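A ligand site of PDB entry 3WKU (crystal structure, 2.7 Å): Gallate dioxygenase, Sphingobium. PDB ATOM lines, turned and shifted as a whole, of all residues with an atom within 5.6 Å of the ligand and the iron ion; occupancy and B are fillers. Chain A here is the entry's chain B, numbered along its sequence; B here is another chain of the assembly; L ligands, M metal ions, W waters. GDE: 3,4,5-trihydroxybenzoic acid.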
ATOM      1  N   HIS A  12      25.659  28.436   3.439  1.00  0.00           N
ATOM      2  CA  HIS A  12      25.161  29.511   4.273  1.00  0.00           C
ATOM      3  C   HIS A  12      24.276  29.064   5.412  1.00  0.00           C
ATOM      4  O   HIS A  12      23.288  29.694   5.663  1.00  0.00           O
ATOM      5  CB  HIS A  12      24.522  30.651   3.455  1.00  0.00           C
ATOM      6  CG  HIS A  12      23.328  30.269   2.627  1.00  0.00           C
ATOM      7  ND1 HIS A  12      23.171  30.708   1.336  1.00  0.00           N
ATOM      8  CD2 HIS A  12      22.231  29.535   2.919  1.00  0.00           C
ATOM      9  CE1 HIS A  12      22.037  30.242   0.846  1.00  0.00           C
ATOM     10  NE2 HIS A  12      21.438  29.516   1.788  1.00  0.00           N
ATOM     11  N   THR A  13      24.661  27.981   6.097  1.00  0.00           N
ATOM     12  CA  THR A  13      23.890  27.389   7.216  1.00  0.00           C
ATOM     13  C   THR A  13      23.915  28.306   8.402  1.00  0.00           C
ATOM     14  O   THR A  13      24.953  28.872   8.722  1.00  0.00           O
ATOM     15  CB  THR A  13      24.572  26.142   7.747  1.00  0.00           C
ATOM     16  OG1 THR A  13      25.473  25.607   6.783  1.00  0.00           O
ATOM     17  CG2 THR A  13      23.580  25.098   8.156  1.00  0.00           C
ATOM     18  N   PRO A  14      22.781  28.432   9.111  1.00  0.00           N
ATOM     19  CA  PRO A  14      22.768  29.219  10.343  1.00  0.00           C
ATOM     20  C   PRO A  14      23.701  28.633  11.379  1.00  0.00           C
ATOM     21  O   PRO A  14      24.076  29.322  12.310  1.00  0.00           O
ATOM     22  CB  PRO A  14      21.315  29.133  10.811  1.00  0.00           C
ATOM     23  CG  PRO A  14      20.751  27.942  10.166  1.00  0.00           C
ATOM     24  CD  PRO A  14      21.463  27.865   8.804  1.00  0.00           C
ATOM     25  N   THR A  15      24.123  27.390  11.184  1.00  0.00           N
ATOM     26  CA  THR A  15      25.048  26.784  12.113  1.00  0.00           C
ATOM     27  C   THR A  15      26.400  27.454  12.078  1.00  0.00           C
ATOM     28  O   THR A  15      27.080  27.537  13.106  1.00  0.00           O
ATOM     29  CB  THR A  15      25.181  25.236  11.966  1.00  0.00           C
ATOM     30  OG1 THR A  15      26.058  24.913  10.875  1.00  0.00           O
ATOM     31  CG2 THR A  15      23.830  24.573  11.766  1.00  0.00           C
ATOM     32  N   ASN A  57      20.032  33.149  -0.927  1.00  0.00           N
ATOM     33  CA  ASN A  57      18.589  33.073  -0.764  1.00  0.00           C
ATOM     34  C   ASN A  57      18.162  33.475   0.637  1.00  0.00           C
ATOM     35  O   ASN A  57      18.786  33.091   1.620  1.00  0.00           O
ATOM     36  CB  ASN A  57      18.001  31.709  -1.180  1.00  0.00           C
ATOM     37  CG  ASN A  57      18.140  30.646  -0.104  1.00  0.00           C
ATOM     38  OD1 ASN A  57      19.234  30.177   0.203  1.00  0.00           O
ATOM     39  ND2 ASN A  57      17.009  30.257   0.491  1.00  0.00           N
ATOM     40  N   HIS A  59      15.471  33.321   3.673  1.00  0.00           N
ATOM     41  CA  HIS A  59      14.762  32.131   4.158  1.00  0.00           C
ATOM     42  C   HIS A  59      13.363  32.396   4.743  1.00  0.00           C
ATOM     43  O   HIS A  59      13.106  32.143   5.914  1.00  0.00           O
ATOM     44  CB  HIS A  59      15.687  31.287   5.039  1.00  0.00           C
ATOM     45  CG  HIS A  59      16.852  30.726   4.274  1.00  0.00           C
ATOM     46  ND1 HIS A  59      17.923  31.498   3.852  1.00  0.00           N
ATOM     47  CD2 HIS A  59      17.085  29.474   3.791  1.00  0.00           C
ATOM     48  CE1 HIS A  59      18.769  30.739   3.182  1.00  0.00           C
ATOM     49  NE2 HIS A  59      18.287  29.514   3.113  1.00  0.00           N
ATOM     50  N   HIS A 124      20.228  34.736   7.466  1.00  0.00           N
ATOM     51  CA  HIS A 124      21.371  33.860   7.518  1.00  0.00           C
ATOM     52  C   HIS A 124      21.943  33.536   6.130  1.00  0.00           C
ATOM     53  O   HIS A 124      23.077  33.122   6.032  1.00  0.00           O
ATOM     54  CB  HIS A 124      21.089  32.596   8.326  1.00  0.00           C
ATOM     55  CG  HIS A 124      20.160  31.618   7.678  1.00  0.00           C
ATOM     56  ND1 HIS A 124      18.841  31.485   8.058  1.00  0.00           N
ATOM     57  CD2 HIS A 124      20.378  30.671   6.740  1.00  0.00           C
ATOM     58  CE1 HIS A 124      18.281  30.520   7.357  1.00  0.00           C
ATOM     59  NE2 HIS A 124      19.195  30.020   6.532  1.00  0.00           N
ATOM     60  N   VAL A 151      14.654  30.688  -4.699  1.00  0.00           N
ATOM     61  CA  VAL A 151      14.773  29.278  -4.997  1.00  0.00           C
ATOM     62  C   VAL A 151      13.846  28.387  -4.137  1.00  0.00           C
ATOM     63  O   VAL A 151      13.997  27.158  -4.125  1.00  0.00           O
ATOM     64  CB  VAL A 151      16.220  28.817  -4.847  1.00  0.00           C
ATOM     65  CG1 VAL A 151      17.127  29.511  -5.857  1.00  0.00           C
ATOM     66  CG2 VAL A 151      16.693  29.068  -3.432  1.00  0.00           C
ATOM     67  N   LEU A 152      12.889  28.990  -3.429  1.00  0.00           N
ATOM     68  CA  LEU A 152      12.179  28.236  -2.404  1.00  0.00           C
ATOM     69  C   LEU A 152      10.768  27.853  -2.781  1.00  0.00           C
ATOM     70  O   LEU A 152      10.257  26.820  -2.334  1.00  0.00           O
ATOM     71  CB  LEU A 152      12.206  28.980  -1.045  1.00  0.00           C
ATOM     72  CG  LEU A 152      13.548  29.071  -0.304  1.00  0.00           C
ATOM     73  CD1 LEU A 152      13.370  29.710   1.067  1.00  0.00           C
ATOM     74  CD2 LEU A 152      14.271  27.722  -0.197  1.00  0.00           C
ATOM     75  N   GLY A 188      25.026  28.648  -0.333  1.00  0.00           N
ATOM     76  CA  GLY A 188      24.005  27.596  -0.231  1.00  0.00           C
ATOM     77  C   GLY A 188      24.499  26.160  -0.438  1.00  0.00           C
ATOM     78  O   GLY A 188      25.523  25.939  -1.072  1.00  0.00           O
ATOM     79  N   GLY A 189      23.764  25.185   0.089  1.00  0.00           N
ATOM     80  CA  GLY A 189      24.141  23.784  -0.004  1.00  0.00           C
ATOM     81  C   GLY A 189      25.403  23.418   0.747  1.00  0.00           C
ATOM     82  O   GLY A 189      25.829  24.171   1.607  1.00  0.00           O
ATOM     83  N   HIS A 192      21.710  18.803   1.596  1.00  0.00           N
ATOM     84  CA  HIS A 192      20.938  18.864   2.821  1.00  0.00           C
ATOM     85  C   HIS A 192      19.451  18.856   2.490  1.00  0.00           C
ATOM     86  O   HIS A 192      19.041  19.420   1.455  1.00  0.00           O
ATOM     87  CB  HIS A 192      21.262  20.124   3.631  1.00  0.00           C
ATOM     88  CG  HIS A 192      20.831  21.408   2.994  1.00  0.00           C
ATOM     89  ND1 HIS A 192      21.610  22.104   2.083  1.00  0.00           N
ATOM     90  CD2 HIS A 192      19.707  22.147   3.158  1.00  0.00           C
ATOM     91  CE1 HIS A 192      20.987  23.201   1.721  1.00  0.00           C
ATOM     92  NE2 HIS A 192      19.824  23.257   2.356  1.00  0.00           N
ATOM     93  N   VAL A 194      16.016  19.791   4.902  1.00  0.00           N
ATOM     94  CA  VAL A 194      15.640  20.249   6.247  1.00  0.00           C
ATOM     95  C   VAL A 194      14.147  20.175   6.541  1.00  0.00           C
ATOM     96  O   VAL A 194      13.652  20.858   7.430  1.00  0.00           O
ATOM     97  CB  VAL A 194      16.174  21.687   6.552  1.00  0.00           C
ATOM     98  CG1 VAL A 194      17.656  21.644   6.890  1.00  0.00           C
ATOM     99  CG2 VAL A 194      15.883  22.617   5.396  1.00  0.00           C
ATOM    100  N   GLU A 239      19.288  24.326  -3.814  1.00  0.00           N
ATOM    101  CA  GLU A 239      19.635  25.753  -3.857  1.00  0.00           C
ATOM    102  C   GLU A 239      20.969  25.963  -4.579  1.00  0.00           C
ATOM    103  O   GLU A 239      21.247  27.063  -5.076  1.00  0.00           O
ATOM    104  CB  GLU A 239      19.578  26.407  -2.459  1.00  0.00           C
ATOM    105  CG  GLU A 239      20.686  26.036  -1.426  1.00  0.00           C
ATOM    106  CD  GLU A 239      20.422  26.597  -0.010  1.00  0.00           C
ATOM    107  OE1 GLU A 239      19.562  27.485   0.144  1.00  0.00           O
ATOM    108  OE2 GLU A 239      21.086  26.185   0.958  1.00  0.00           O
ATOM    109  N   MET A 242      22.549  28.428  -7.293  1.00  0.00           N
ATOM    110  CA  MET A 242      23.217  29.725  -7.111  1.00  0.00           C
ATOM    111  C   MET A 242      24.717  29.615  -7.335  1.00  0.00           C
ATOM    112  O   MET A 242      25.371  30.596  -7.665  1.00  0.00           O
ATOM    113  CB  MET A 242      22.907  30.320  -5.723  1.00  0.00           C
ATOM    114  CG  MET A 242      21.479  30.826  -5.611  1.00  0.00           C
ATOM    115  SD  MET A 242      20.929  31.251  -3.947  1.00  0.00           S
ATOM    116  CE  MET A 242      20.950  29.680  -3.131  1.00  0.00           C
ATOM    117  N   MET A 266      23.489  18.506   9.538  1.00  0.00           N
ATOM    118  CA  MET A 266      22.517  18.356   8.445  1.00  0.00           C
ATOM    119  C   MET A 266      23.017  18.803   7.074  1.00  0.00           C
ATOM    120  O   MET A 266      22.421  18.464   6.066  1.00  0.00           O
ATOM    121  CB  MET A 266      21.266  19.200   8.725  1.00  0.00           C
ATOM    122  CG  MET A 266      20.596  18.988  10.085  1.00  0.00           C
ATOM    123  SD  MET A 266      19.562  17.516  10.074  1.00  0.00           S
ATOM    124  CE  MET A 266      18.211  18.116   9.026  1.00  0.00           C
ATOM    125  N   THR A 267      24.062  19.620   7.035  1.00  0.00           N
ATOM    126  CA  THR A 267      24.434  20.332   5.822  1.00  0.00           C
ATOM    127  C   THR A 267      25.875  20.111   5.427  1.00  0.00           C
ATOM    128  O   THR A 267      26.774  20.230   6.234  1.00  0.00           O
ATOM    129  CB  THR A 267      24.261  21.851   6.019  1.00  0.00           C
ATOM    130  OG1 THR A 267      23.066  22.106   6.773  1.00  0.00           O
ATOM    131  CG2 THR A 267      24.234  22.605   4.647  1.00  0.00           C
ATOM    132  N   PHE B 373       9.402  25.092   5.779  1.00  0.00           N
ATOM    133  CA  PHE B 373      10.199  24.815   6.963  1.00  0.00           C
ATOM    134  C   PHE B 373      10.610  26.086   7.720  1.00  0.00           C
ATOM    135  O   PHE B 373      10.688  26.122   8.951  1.00  0.00           O
ATOM    136  CB  PHE B 373      11.445  24.037   6.567  1.00  0.00           C
ATOM    137  CG  PHE B 373      12.469  23.938   7.659  1.00  0.00           C
ATOM    138  CD1 PHE B 373      12.209  23.192   8.803  1.00  0.00           C
ATOM    139  CD2 PHE B 373      13.684  24.600   7.550  1.00  0.00           C
ATOM    140  CE1 PHE B 373      13.136  23.104   9.823  1.00  0.00           C
ATOM    141  CE2 PHE B 373      14.616  24.517   8.546  1.00  0.00           C
ATOM    142  CZ  PHE B 373      14.345  23.763   9.686  1.00  0.00           C
ATOM    143  N   PHE B 374      10.852  27.136   6.966  1.00  0.00           N
ATOM    144  CA  PHE B 374      11.523  28.285   7.494  1.00  0.00           C
ATOM    145  C   PHE B 374      10.721  29.128   8.496  1.00  0.00           C
ATOM    146  O   PHE B 374      11.322  29.810   9.326  1.00  0.00           O
ATOM    147  CB  PHE B 374      12.105  29.107   6.355  1.00  0.00           C
ATOM    148  CG  PHE B 374      13.056  28.337   5.505  1.00  0.00           C
ATOM    149  CD1 PHE B 374      14.292  27.962   6.000  1.00  0.00           C
ATOM    150  CD2 PHE B 374      12.704  27.937   4.222  1.00  0.00           C
ATOM    151  CE1 PHE B 374      15.194  27.204   5.228  1.00  0.00           C
ATOM    152  CE2 PHE B 374      13.581  27.206   3.423  1.00  0.00           C
ATOM    153  CZ  PHE B 374      14.833  26.826   3.930  1.00  0.00           C
ATOM    154  N   GLU B 377      11.196  27.142  11.595  1.00  0.00           N
ATOM    155  CA  GLU B 377      12.491  27.613  12.139  1.00  0.00           C
ATOM    156  C   GLU B 377      12.377  28.759  13.175  1.00  0.00           C
ATOM    157  O   GLU B 377      12.944  28.690  14.263  1.00  0.00           O
ATOM    158  CB  GLU B 377      13.443  28.047  11.006  1.00  0.00           C
ATOM    159  CG  GLU B 377      14.936  28.090  11.413  1.00  0.00           C
ATOM    160  CD  GLU B 377      15.905  28.050  10.231  1.00  0.00           C
ATOM    161  OE1 GLU B 377      15.692  28.761   9.211  1.00  0.00           O
ATOM    162  OE2 GLU B 377      16.905  27.313  10.326  1.00  0.00           O
ATOM    163  N   ASN B 387      16.617  23.827  15.982  1.00  0.00           N
ATOM    164  CA  ASN B 387      16.274  23.199  14.713  1.00  0.00           C
ATOM    165  C   ASN B 387      16.237  21.668  14.769  1.00  0.00           C
ATOM    166  O   ASN B 387      15.395  21.048  14.118  1.00  0.00           O
ATOM    167  CB  ASN B 387      17.248  23.632  13.619  1.00  0.00           C
ATOM    168  CG  ASN B 387      17.292  25.133  13.432  1.00  0.00           C
ATOM    169  OD1 ASN B 387      17.851  25.837  14.241  1.00  0.00           O
ATOM    170  ND2 ASN B 387      16.743  25.606  12.333  1.00  0.00           N
ATOM    171  N   TYR B 391      13.769  18.729  13.608  1.00  0.00           N
ATOM    172  CA  TYR B 391      14.218  17.702  12.701  1.00  0.00           C
ATOM    173  C   TYR B 391      13.892  16.328  13.261  1.00  0.00           C
ATOM    174  O   TYR B 391      13.515  15.407  12.524  1.00  0.00           O
ATOM    175  CB  TYR B 391      15.716  17.846  12.443  1.00  0.00           C
ATOM    176  CG  TYR B 391      16.128  19.144  11.780  1.00  0.00           C
ATOM    177  CD1 TYR B 391      15.271  19.791  10.910  1.00  0.00           C
ATOM    178  CD2 TYR B 391      17.353  19.731  12.014  1.00  0.00           C
ATOM    179  CE1 TYR B 391      15.635  20.965  10.295  1.00  0.00           C
ATOM    180  CE2 TYR B 391      17.723  20.924  11.396  1.00  0.00           C
ATOM    181  CZ  TYR B 391      16.849  21.524  10.535  1.00  0.00           C
ATOM    182  OH  TYR B 391      17.149  22.728   9.896  1.00  0.00           O
ATOM    183  N   TYR B 412      21.627  24.384  18.159  1.00  0.00           N
ATOM    184  CA  TYR B 412      21.600  25.751  17.608  1.00  0.00           C
ATOM    185  C   TYR B 412      20.169  26.120  17.200  1.00  0.00           C
ATOM    186  O   TYR B 412      19.315  25.242  17.079  1.00  0.00           O
ATOM    187  CB  TYR B 412      22.481  25.817  16.356  1.00  0.00           C
ATOM    188  CG  TYR B 412      22.045  24.902  15.216  1.00  0.00           C
ATOM    189  CD1 TYR B 412      21.176  25.341  14.217  1.00  0.00           C
ATOM    190  CD2 TYR B 412      22.530  23.591  15.122  1.00  0.00           C
ATOM    191  CE1 TYR B 412      20.796  24.506  13.148  1.00  0.00           C
ATOM    192  CE2 TYR B 412      22.142  22.749  14.064  1.00  0.00           C
ATOM    193  CZ  TYR B 412      21.282  23.214  13.097  1.00  0.00           C
ATOM    194  OH  TYR B 412      20.913  22.398  12.038  1.00  0.00           O
HETATM  195  OAA GDE L   1      19.519  23.109   9.523  1.00  0.00           O
HETATM  196  OAB GDE L   1      21.608  23.288   8.926  1.00  0.00           O
HETATM  197  OAC GDE L   1      17.594  27.314   7.436  1.00  0.00           O
HETATM  198  OAD GDE L   1      21.058  25.931   4.529  1.00  0.00           O
HETATM  199  OAE GDE L   1      19.038  27.553   5.024  1.00  0.00           O
HETATM  200  CAF GDE L   1      18.999  25.522   8.069  1.00  0.00           C
HETATM  201  CAG GDE L   1      20.764  24.792   6.626  1.00  0.00           C
HETATM  202  CAH GDE L   1      20.415  23.628   8.813  1.00  0.00           C
HETATM  203  CAI GDE L   1      18.647  26.489   7.145  1.00  0.00           C
HETATM  204  CAJ GDE L   1      20.395  25.776   5.697  1.00  0.00           C
HETATM  205  CAK GDE L   1      20.065  24.675   7.807  1.00  0.00           C
HETATM  206  CAL GDE L   1      19.350  26.615   5.962  1.00  0.00           C
HETATM  207 FE    FE M   1      19.426  28.756   1.385  1.00  0.00          FE
HETATM  208  O   HOH W   1      18.767  26.123   2.833  1.00  0.00           O
HETATM  209  O   HOH W   2      17.686  27.763   1.407  1.00  0.00           O
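The side-chain carboxylate of Glu 377 of chain B lies within hydrogen-bond range of an oxygen (OAC) of the ligand, at 3.0 Å.
The side-chain hydroxyl of Tyr 412 of chain B sits at hydrogen-bond distance from an oxygen (OAA) of the ligand.
The side-chain hydroxyl of Tyr 391 of chain B sits at hydrogen-bond distance from an oxygen (OAA) of the ligand (2.4 Å).
A ring nitrogen (NE2) of His 59 lies close to an oxygen (OAE) of the ligand (2.8 Å).
OAB of the ligand sits at hydrogen-bond distance from OG1 of Thr 267 (2.9 Å).
A ring nitrogen (NE2) of His 124 is in hydrogen-bond range of an oxygen (OAE) of the ligand, 2.9 Å away.
Thr 13 touches the ligand.
CD of Pro 14 touches CAF of the ligand, at 3.5 Å.
CG2 of Thr 15 touches OAB of the ligand, at 3.8 Å.
His 192 touches the ligand (NE2 to OAD, 3.7 Å).
CG1 of Val 194 touches OAA of the ligand, 3.5 Å away.
CE1 of Phe 374 of chain B touches OAC of the ligand, 3.3 Å away.
Hydrophobic or aromatic side chains within 4 Å of the ligand: Pro 14, His 59, His 124, His 192, Val 194, Phe 374 of chain B, Tyr 391 of chain B and Tyr 412 of chain B.
Of the 23 residues printed, 13 come within 4 Å of the ligand.
The nearest printed residue that does not touch the ligand is Met 266 (4.1 Å).
OE1 of Glu 239 is bound to the iron ion (1.8 Å).
The iron ion is bound by OD1 of Asn 57 (1.9 Å).
Water W2 is bound to the iron ion (2.0 Å).
A ring nitrogen (NE2) of His 12 is bound to the iron ion, at 2.2 Å.
NE2 of His 59 is bound to the iron ion.
The iron ion has five donor atoms within binding distance.
Water W1 lies within hydrogen-bond range of OAE of the ligand, OE2 of Glu 239 and NE2 of His 192.
The side-chain carboxylate (OE2) of Glu 239 sits at hydrogen-bond distance from the backbone NH (N) of Gly 189 (3.0 Å).
The side-chain carboxylate (OE2) of Glu 377 of chain B is in hydrogen-bond range of the side-chain amide nitrogen (ND2) of Asn 387 of chain B (2.6 Å).
The side-chain sulfur (SD) of Met 242 is in hydrogen-bond range of the backbone NH (N) of Asn 57 (3.7 Å).
A ring nitrogen (NE2) of His 192 sits close to the side-chain carboxylate of Glu 239, at 3.5 Å.
N of Gly 188 lies within hydrogen-bond range of ND1 of His 12 (3.2 Å).
A ring nitrogen (ND1) of His 59 lies within hydrogen-bond range of a ring nitrogen (NE2) of His 124.
The backbone carbonyl oxygen (O) of Tyr 412 of chain B sits at hydrogen-bond distance from the backbone NH (N) of Asn 387 of chain B, at 3.2 Å.
Within 4 Å of the iron ion: His 12, Asn 57, His 59 and Glu 239.
The nearest printed residue that does not touch the iron ion is Met 242 (4.9 Å).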
